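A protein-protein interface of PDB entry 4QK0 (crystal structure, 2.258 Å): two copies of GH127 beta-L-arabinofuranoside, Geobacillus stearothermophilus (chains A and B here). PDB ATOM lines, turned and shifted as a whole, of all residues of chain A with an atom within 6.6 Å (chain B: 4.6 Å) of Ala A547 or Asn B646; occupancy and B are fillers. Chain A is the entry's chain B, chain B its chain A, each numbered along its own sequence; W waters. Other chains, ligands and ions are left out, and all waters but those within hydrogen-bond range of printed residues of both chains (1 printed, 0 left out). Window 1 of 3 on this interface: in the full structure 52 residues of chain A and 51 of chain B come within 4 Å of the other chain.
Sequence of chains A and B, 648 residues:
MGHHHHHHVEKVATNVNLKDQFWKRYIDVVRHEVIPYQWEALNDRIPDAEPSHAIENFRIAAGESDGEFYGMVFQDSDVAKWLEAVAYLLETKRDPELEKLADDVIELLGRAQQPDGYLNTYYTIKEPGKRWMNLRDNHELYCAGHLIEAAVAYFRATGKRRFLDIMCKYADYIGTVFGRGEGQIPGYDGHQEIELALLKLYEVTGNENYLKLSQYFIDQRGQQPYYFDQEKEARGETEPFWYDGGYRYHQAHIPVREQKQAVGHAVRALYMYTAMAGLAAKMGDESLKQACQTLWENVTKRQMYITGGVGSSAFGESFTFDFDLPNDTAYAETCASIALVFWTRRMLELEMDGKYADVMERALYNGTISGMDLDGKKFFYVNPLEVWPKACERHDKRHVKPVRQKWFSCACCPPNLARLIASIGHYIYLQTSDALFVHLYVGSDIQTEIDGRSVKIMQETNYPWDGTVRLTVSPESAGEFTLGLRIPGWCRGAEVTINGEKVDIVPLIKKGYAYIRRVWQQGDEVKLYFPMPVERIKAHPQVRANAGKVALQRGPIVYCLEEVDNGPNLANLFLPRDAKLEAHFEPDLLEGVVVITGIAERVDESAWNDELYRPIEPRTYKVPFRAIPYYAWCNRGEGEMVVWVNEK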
ATOM      1  N   LYS A 538       7.687 -34.060 -13.451  1.00  0.00           N
ATOM      2  CA  LYS A 538       6.807 -32.988 -13.158  1.00  0.00           C
ATOM      3  C   LYS A 538       7.053 -32.444 -11.764  1.00  0.00           C
ATOM      4  O   LYS A 538       7.315 -33.186 -10.824  1.00  0.00           O
ATOM      5  CB  LYS A 538       5.342 -33.433 -13.219  1.00  0.00           C
ATOM      6  CG  LYS A 538       4.893 -33.863 -14.577  1.00  0.00           C
ATOM      7  CD  LYS A 538       4.793 -32.723 -15.631  1.00  0.00           C
ATOM      8  CE  LYS A 538       3.903 -31.568 -15.153  1.00  0.00           C
ATOM      9  NZ  LYS A 538       3.786 -30.414 -16.086  1.00  0.00           N
ATOM     10  N   ALA A 539       6.973 -31.124 -11.635  1.00  0.00           N
ATOM     11  CA  ALA A 539       7.126 -30.511 -10.320  1.00  0.00           C
ATOM     12  C   ALA A 539       5.792 -30.381  -9.628  1.00  0.00           C
ATOM     13  O   ALA A 539       4.754 -30.227 -10.258  1.00  0.00           O
ATOM     14  CB  ALA A 539       7.773 -29.155 -10.421  1.00  0.00           C
ATOM     15  N   HIS A 540       5.828 -30.401  -8.303  1.00  0.00           N
ATOM     16  CA  HIS A 540       4.650 -30.190  -7.515  1.00  0.00           C
ATOM     17  C   HIS A 540       3.904 -28.932  -8.070  1.00  0.00           C
ATOM     18  O   HIS A 540       4.536 -27.939  -8.422  1.00  0.00           O
ATOM     19  CB  HIS A 540       5.081 -29.970  -6.078  1.00  0.00           C
ATOM     20  CG  HIS A 540       3.959 -29.983  -5.094  1.00  0.00           C
ATOM     21  ND1 HIS A 540       2.998 -29.006  -5.053  1.00  0.00           N
ATOM     22  CD2 HIS A 540       3.680 -30.822  -4.072  1.00  0.00           C
ATOM     23  CE1 HIS A 540       2.176 -29.239  -4.045  1.00  0.00           C
ATOM     24  NE2 HIS A 540       2.559 -30.352  -3.449  1.00  0.00           N
ATOM     25  N   PRO A 541       2.584 -28.990  -8.144  1.00  0.00           N
ATOM     26  CA  PRO A 541       1.808 -27.874  -8.686  1.00  0.00           C
ATOM     27  C   PRO A 541       1.980 -26.541  -8.004  1.00  0.00           C
ATOM     28  O   PRO A 541       1.670 -25.552  -8.596  1.00  0.00           O
ATOM     29  CB  PRO A 541       0.358 -28.340  -8.539  1.00  0.00           C
ATOM     30  CG  PRO A 541       0.439 -29.804  -8.530  1.00  0.00           C
ATOM     31  CD  PRO A 541       1.713 -30.145  -7.816  1.00  0.00           C
ATOM     32  N   VAL A 543       4.833 -25.324  -7.329  1.00  0.00           N
ATOM     33  CA  VAL A 543       5.956 -24.713  -8.027  1.00  0.00           C
ATOM     34  C   VAL A 543       5.508 -23.949  -9.306  1.00  0.00           C
ATOM     35  O   VAL A 543       5.416 -24.490 -10.394  1.00  0.00           O
ATOM     36  CB  VAL A 543       7.050 -25.712  -8.381  1.00  0.00           C
ATOM     37  CG1 VAL A 543       8.245 -24.953  -8.964  1.00  0.00           C
ATOM     38  CG2 VAL A 543       7.515 -26.447  -7.134  1.00  0.00           C
ATOM     39  N   ARG A 544       5.228 -22.682  -9.110  1.00  0.00           N
ATOM     40  CA  ARG A 544       4.658 -21.832 -10.118  1.00  0.00           C
ATOM     41  C   ARG A 544       5.509 -21.761 -11.341  1.00  0.00           C
ATOM     42  O   ARG A 544       5.011 -21.843 -12.414  1.00  0.00           O
ATOM     43  CB  ARG A 544       4.514 -20.400  -9.589  1.00  0.00           C
ATOM     44  CG  ARG A 544       3.186 -20.012  -8.988  1.00  0.00           C
ATOM     45  CD  ARG A 544       2.999 -20.695  -7.673  1.00  0.00           C
ATOM     46  NE  ARG A 544       1.851 -20.144  -7.000  1.00  0.00           N
ATOM     47  CZ  ARG A 544       1.344 -20.662  -5.901  1.00  0.00           C
ATOM     48  NH1 ARG A 544       1.868 -21.757  -5.362  1.00  0.00           N
ATOM     49  NH2 ARG A 544       0.275 -20.110  -5.374  1.00  0.00           N
ATOM     50  N   ALA A 545       6.816 -21.672 -11.168  1.00  0.00           N
ATOM     51  CA  ALA A 545       7.696 -21.579 -12.298  1.00  0.00           C
ATOM     52  C   ALA A 545       7.560 -22.737 -13.296  1.00  0.00           C
ATOM     53  O   ALA A 545       7.930 -22.556 -14.425  1.00  0.00           O
ATOM     54  CB  ALA A 545       9.128 -21.475 -11.840  1.00  0.00           C
ATOM     55  N   ASN A 546       7.025 -23.892 -12.892  1.00  0.00           N
ATOM     56  CA  ASN A 546       7.073 -25.060 -13.739  1.00  0.00           C
ATOM     57  C   ASN A 546       5.747 -25.562 -14.126  1.00  0.00           C
ATOM     58  O   ASN A 546       5.607 -26.640 -14.716  1.00  0.00           O
ATOM     59  CB  ASN A 546       7.929 -26.167 -13.102  1.00  0.00           C
ATOM     60  CG  ASN A 546       9.367 -25.755 -12.949  1.00  0.00           C
ATOM     61  OD1 ASN A 546       9.897 -24.987 -13.762  1.00  0.00           O
ATOM     62  ND2 ASN A 546       9.992 -26.162 -11.859  1.00  0.00           N
ATOM     63  N   ALA A 547       4.737 -24.766 -13.808  1.00  0.00           N
ATOM     64  CA  ALA A 547       3.376 -25.010 -14.309  1.00  0.00           C
ATOM     65  C   ALA A 547       3.485 -25.164 -15.788  1.00  0.00           C
ATOM     66  O   ALA A 547       4.080 -24.321 -16.441  1.00  0.00           O
ATOM     67  CB  ALA A 547       2.487 -23.795 -13.977  1.00  0.00           C
ATOM     68  N   GLY A 548       2.892 -26.205 -16.325  1.00  0.00           N
ATOM     69  CA  GLY A 548       2.881 -26.447 -17.751  1.00  0.00           C
ATOM     70  C   GLY A 548       4.224 -26.840 -18.347  1.00  0.00           C
ATOM     71  O   GLY A 548       4.374 -26.881 -19.597  1.00  0.00           O
ATOM     72  N   LYS A 549       5.183 -27.210 -17.501  1.00  0.00           N
ATOM     73  CA  LYS A 549       6.470 -27.645 -17.996  1.00  0.00           C
ATOM     74  C   LYS A 549       6.858 -29.007 -17.514  1.00  0.00           C
ATOM     75  O   LYS A 549       6.349 -29.482 -16.519  1.00  0.00           O
ATOM     76  CB  LYS A 549       7.521 -26.652 -17.560  1.00  0.00           C
ATOM     77  CG  LYS A 549       7.263 -25.240 -18.012  1.00  0.00           C
ATOM     78  CD  LYS A 549       8.477 -24.425 -17.663  1.00  0.00           C
ATOM     79  CE  LYS A 549       8.263 -22.940 -17.643  1.00  0.00           C
ATOM     80  NZ  LYS A 549       8.222 -22.425 -19.022  1.00  0.00           N
ATOM     81  N   ASN A 646       8.370 -26.539 -22.042  1.00  0.00           N
ATOM     82  CA  ASN A 646       6.936 -26.456 -22.173  1.00  0.00           C
ATOM     83  C   ASN A 646       6.347 -27.710 -22.723  1.00  0.00           C
ATOM     84  O   ASN A 646       6.876 -28.318 -23.591  1.00  0.00           O
ATOM     85  CB  ASN A 646       6.499 -25.260 -23.010  1.00  0.00           C
ATOM     86  CG  ASN A 646       6.685 -23.957 -22.305  1.00  0.00           C
ATOM     87  OD1 ASN A 646       7.405 -23.111 -22.757  1.00  0.00           O
ATOM     88  ND2 ASN A 646       6.047 -23.806 -21.194  1.00  0.00           N
ATOM     89  N   GLY B 548       3.251 -20.598 -24.595  1.00  0.00           N
ATOM     90  CA  GLY B 548       2.225 -21.446 -24.005  1.00  0.00           C
ATOM     91  C   GLY B 548       1.117 -20.754 -23.224  1.00  0.00           C
ATOM     92  O   GLY B 548       0.386 -21.412 -22.469  1.00  0.00           O
ATOM     93  N   LYS B 549       1.017 -19.436 -23.354  1.00  0.00           N
ATOM     94  CA  LYS B 549       0.036 -18.679 -22.596  1.00  0.00           C
ATOM     95  C   LYS B 549      -0.861 -17.890 -23.484  1.00  0.00           C
ATOM     96  O   LYS B 549      -0.516 -17.625 -24.603  1.00  0.00           O
ATOM     97  CB  LYS B 549       0.682 -17.755 -21.616  1.00  0.00           C
ATOM     98  CG  LYS B 549       1.594 -18.442 -20.638  1.00  0.00           C
ATOM     99  CD  LYS B 549       1.963 -17.388 -19.597  1.00  0.00           C
ATOM    100  CE  LYS B 549       3.183 -17.731 -18.783  1.00  0.00           C
ATOM    101  NZ  LYS B 549       2.811 -18.712 -17.752  1.00  0.00           N
ATOM    102  N   ALA B 571      -1.293 -19.957 -11.575  1.00  0.00           N
ATOM    103  CA  ALA B 571      -0.384 -20.649 -12.542  1.00  0.00           C
ATOM    104  C   ALA B 571      -0.871 -22.055 -12.848  1.00  0.00           C
ATOM    105  O   ALA B 571      -0.723 -22.540 -13.967  1.00  0.00           O
ATOM    106  CB  ALA B 571       1.032 -20.705 -12.001  1.00  0.00           C
ATOM    107  N   LEU B 573      -3.791 -23.137 -13.578  1.00  0.00           N
ATOM    108  CA  LEU B 573      -5.066 -23.013 -14.300  1.00  0.00           C
ATOM    109  C   LEU B 573      -4.705 -23.041 -15.745  1.00  0.00           C
ATOM    110  O   LEU B 573      -3.822 -22.304 -16.178  1.00  0.00           O
ATOM    111  CB  LEU B 573      -5.758 -21.684 -14.054  1.00  0.00           C
ATOM    112  CG  LEU B 573      -6.959 -21.600 -13.116  1.00  0.00           C
ATOM    113  CD1 LEU B 573      -7.477 -20.172 -13.117  1.00  0.00           C
ATOM    114  CD2 LEU B 573      -8.083 -22.505 -13.520  1.00  0.00           C
ATOM    115  N   PHE B 574      -5.373 -23.907 -16.476  1.00  0.00           N
ATOM    116  CA  PHE B 574      -5.084 -24.174 -17.854  1.00  0.00           C
ATOM    117  C   PHE B 574      -6.378 -23.973 -18.626  1.00  0.00           C
ATOM    118  O   PHE B 574      -7.430 -24.520 -18.275  1.00  0.00           O
ATOM    119  CB  PHE B 574      -4.496 -25.591 -18.034  1.00  0.00           C
ATOM    120  CG  PHE B 574      -3.199 -25.790 -17.293  1.00  0.00           C
ATOM    121  CD1 PHE B 574      -3.188 -26.082 -15.933  1.00  0.00           C
ATOM    122  CD2 PHE B 574      -1.993 -25.634 -17.943  1.00  0.00           C
ATOM    123  CE1 PHE B 574      -1.999 -26.231 -15.244  1.00  0.00           C
ATOM    124  CE2 PHE B 574      -0.808 -25.773 -17.276  1.00  0.00           C
ATOM    125  CZ  PHE B 574      -0.807 -26.077 -15.908  1.00  0.00           C
ATOM    126  N   LEU B 575      -6.297 -23.160 -19.671  1.00  0.00           N
ATOM    127  CA  LEU B 575      -7.456 -22.853 -20.463  1.00  0.00           C
ATOM    128  C   LEU B 575      -7.356 -23.674 -21.693  1.00  0.00           C
ATOM    129  O   LEU B 575      -6.489 -23.430 -22.513  1.00  0.00           O
ATOM    130  CB  LEU B 575      -7.484 -21.343 -20.769  1.00  0.00           C
ATOM    131  CG  LEU B 575      -8.705 -20.878 -21.555  1.00  0.00           C
ATOM    132  CD1 LEU B 575      -9.998 -21.114 -20.773  1.00  0.00           C
ATOM    133  CD2 LEU B 575      -8.642 -19.391 -21.894  1.00  0.00           C
ATOM    134  N   TRP B 644      -1.833 -13.382 -18.348  1.00  0.00           N
ATOM    135  CA  TRP B 644      -1.480 -14.398 -19.272  1.00  0.00           C
ATOM    136  C   TRP B 644      -1.689 -15.751 -18.600  1.00  0.00           C
ATOM    137  O   TRP B 644      -0.954 -16.130 -17.691  1.00  0.00           O
ATOM    138  CB  TRP B 644      -0.043 -14.200 -19.744  1.00  0.00           C
ATOM    139  CG  TRP B 644       0.064 -13.044 -20.624  1.00  0.00           C
ATOM    140  CD1 TRP B 644       0.429 -11.771 -20.285  1.00  0.00           C
ATOM    141  CD2 TRP B 644      -0.178 -13.034 -22.024  1.00  0.00           C
ATOM    142  NE1 TRP B 644       0.382 -10.974 -21.370  1.00  0.00           N
ATOM    143  CE2 TRP B 644       0.040 -11.734 -22.465  1.00  0.00           C
ATOM    144  CE3 TRP B 644      -0.549 -14.011 -22.949  1.00  0.00           C
ATOM    145  CZ2 TRP B 644      -0.111 -11.361 -23.798  1.00  0.00           C
ATOM    146  CZ3 TRP B 644      -0.669 -13.657 -24.263  1.00  0.00           C
ATOM    147  CH2 TRP B 644      -0.478 -12.318 -24.677  1.00  0.00           C
ATOM    148  N   VAL B 645      -2.643 -16.505 -19.087  1.00  0.00           N
ATOM    149  CA  VAL B 645      -2.941 -17.807 -18.506  1.00  0.00           C
ATOM    150  C   VAL B 645      -2.404 -18.950 -19.363  1.00  0.00           C
ATOM    151  O   VAL B 645      -2.395 -18.862 -20.593  1.00  0.00           O
ATOM    152  CB  VAL B 645      -4.432 -17.930 -18.020  1.00  0.00           C
ATOM    153  CG1 VAL B 645      -5.272 -16.716 -18.288  1.00  0.00           C
ATOM    154  CG2 VAL B 645      -5.139 -19.181 -18.455  1.00  0.00           C
ATOM    155  N   ASN B 646      -1.911 -19.981 -18.705  1.00  0.00           N
ATOM    156  CA  ASN B 646      -1.483 -21.180 -19.364  1.00  0.00           C
ATOM    157  C   ASN B 646      -2.545 -21.827 -20.199  1.00  0.00           C
ATOM    158  O   ASN B 646      -3.657 -21.928 -19.810  1.00  0.00           O
ATOM    159  CB  ASN B 646      -0.935 -22.203 -18.387  1.00  0.00           C
ATOM    160  CG  ASN B 646       0.352 -21.799 -17.797  1.00  0.00           C
ATOM    161  OD1 ASN B 646       0.442 -21.642 -16.637  1.00  0.00           O
ATOM    162  ND2 ASN B 646       1.335 -21.634 -18.590  1.00  0.00           N
ATOM    163  N   GLU B 647      -2.143 -22.265 -21.359  1.00  0.00           N
ATOM    164  CA  GLU B 647      -3.032 -22.821 -22.323  1.00  0.00           C
ATOM    165  C   GLU B 647      -3.011 -24.337 -22.330  1.00  0.00           C
ATOM    166  O   GLU B 647      -2.007 -24.946 -22.142  1.00  0.00           O
ATOM    167  CB  GLU B 647      -2.696 -22.221 -23.689  1.00  0.00           C
ATOM    168  CG  GLU B 647      -3.567 -22.596 -24.853  1.00  0.00           C
ATOM    169  CD  GLU B 647      -3.668 -21.524 -25.940  1.00  0.00           C
ATOM    170  OE1 GLU B 647      -2.677 -21.219 -26.604  1.00  0.00           O
ATOM    171  OE2 GLU B 647      -4.763 -21.004 -26.151  1.00  0.00           O
ATOM    172  N   LYS B 648      -4.189 -24.904 -22.487  1.00  0.00           N
ATOM    173  CA  LYS B 648      -4.477 -26.303 -22.801  1.00  0.00           C
ATOM    174  C   LYS B 648      -3.855 -27.384 -21.968  1.00  0.00           C
ATOM    175  O   LYS B 648      -4.577 -28.183 -21.392  1.00  0.00           O
ATOM    176  CB  LYS B 648      -4.315 -26.582 -24.286  1.00  0.00           C
ATOM    177  CG  LYS B 648      -2.982 -27.167 -24.677  1.00  0.00           C
ATOM    178  CD  LYS B 648      -3.152 -28.324 -25.643  1.00  0.00           C
ATOM    179  CE  LYS B 648      -2.391 -29.558 -25.186  1.00  0.00           C
ATOM    180  NZ  LYS B 648      -3.321 -30.684 -24.961  1.00  0.00           N
HETATM  181  O   HOH W   1       0.145 -18.868  -8.873  1.00  0.00           O
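3 positions are printed for both chains.
Water W1 lies within hydrogen-bond range of NE of Arg A544 (2.8 Å) and N of Ala B571 (3.2 Å).
Ala B571 touches Arg A544 (CB to CG, 3.8 Å).
Ala A547 touches Ala B571 (CB to O, 3.4 Å).
Ala A547 touches Asn B646.
Phe B574 touches Gly A548 (CZ to N, 3.7 Å).
Hydrophobic or aromatic side chains of chain B that line the printed part of chain A: Ala B571 and Phe B574.
Of the 12 printed residues of chain A, 3 touch a printed residue of chain B.
Printed residues of chain A that touch a printed residue of chain B: Arg A544, Ala A547 and Gly A548.
Hydrophobic or aromatic side chains of chain A within 4 Å of the printed part of chain B: Ala A547.
Among the printed residues, no Asp or Glu carboxylate lies within 4 Å of a Lys or Arg side-chain nitrogen of the other chain.
Of the printed residues of chain A, Asn B646 touches Ala A547.
Of the printed residues of chain A, Ala B571 touches Arg A544 (3.8 Å) and Ala A547 (3.4 Å).
Of the printed residues of chain B, Arg A544 touches Ala B571 (3.8 Å).
Of the printed residues of chain A, Phe B574 touches Gly A548.
Of the printed residues of chain B, Gly A548 touches Phe B574 (3.7 Å).
The nearest printed residue of chain B that does not touch Ala A547 is Phe B574 (4.4 Å).
The backbone NH (N) of Leu B575 sits at hydrogen-bond distance from the backbone carbonyl oxygen (O) of Asn B646 (2.9 Å).
The backbone carbonyl oxygen of Ala B571 lies close to the side-chain amide oxygen of Asn B646 (3.0 Å).
NZ of Lys B549 sits close to ND2 of Asn B646, 3.4 Å away.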
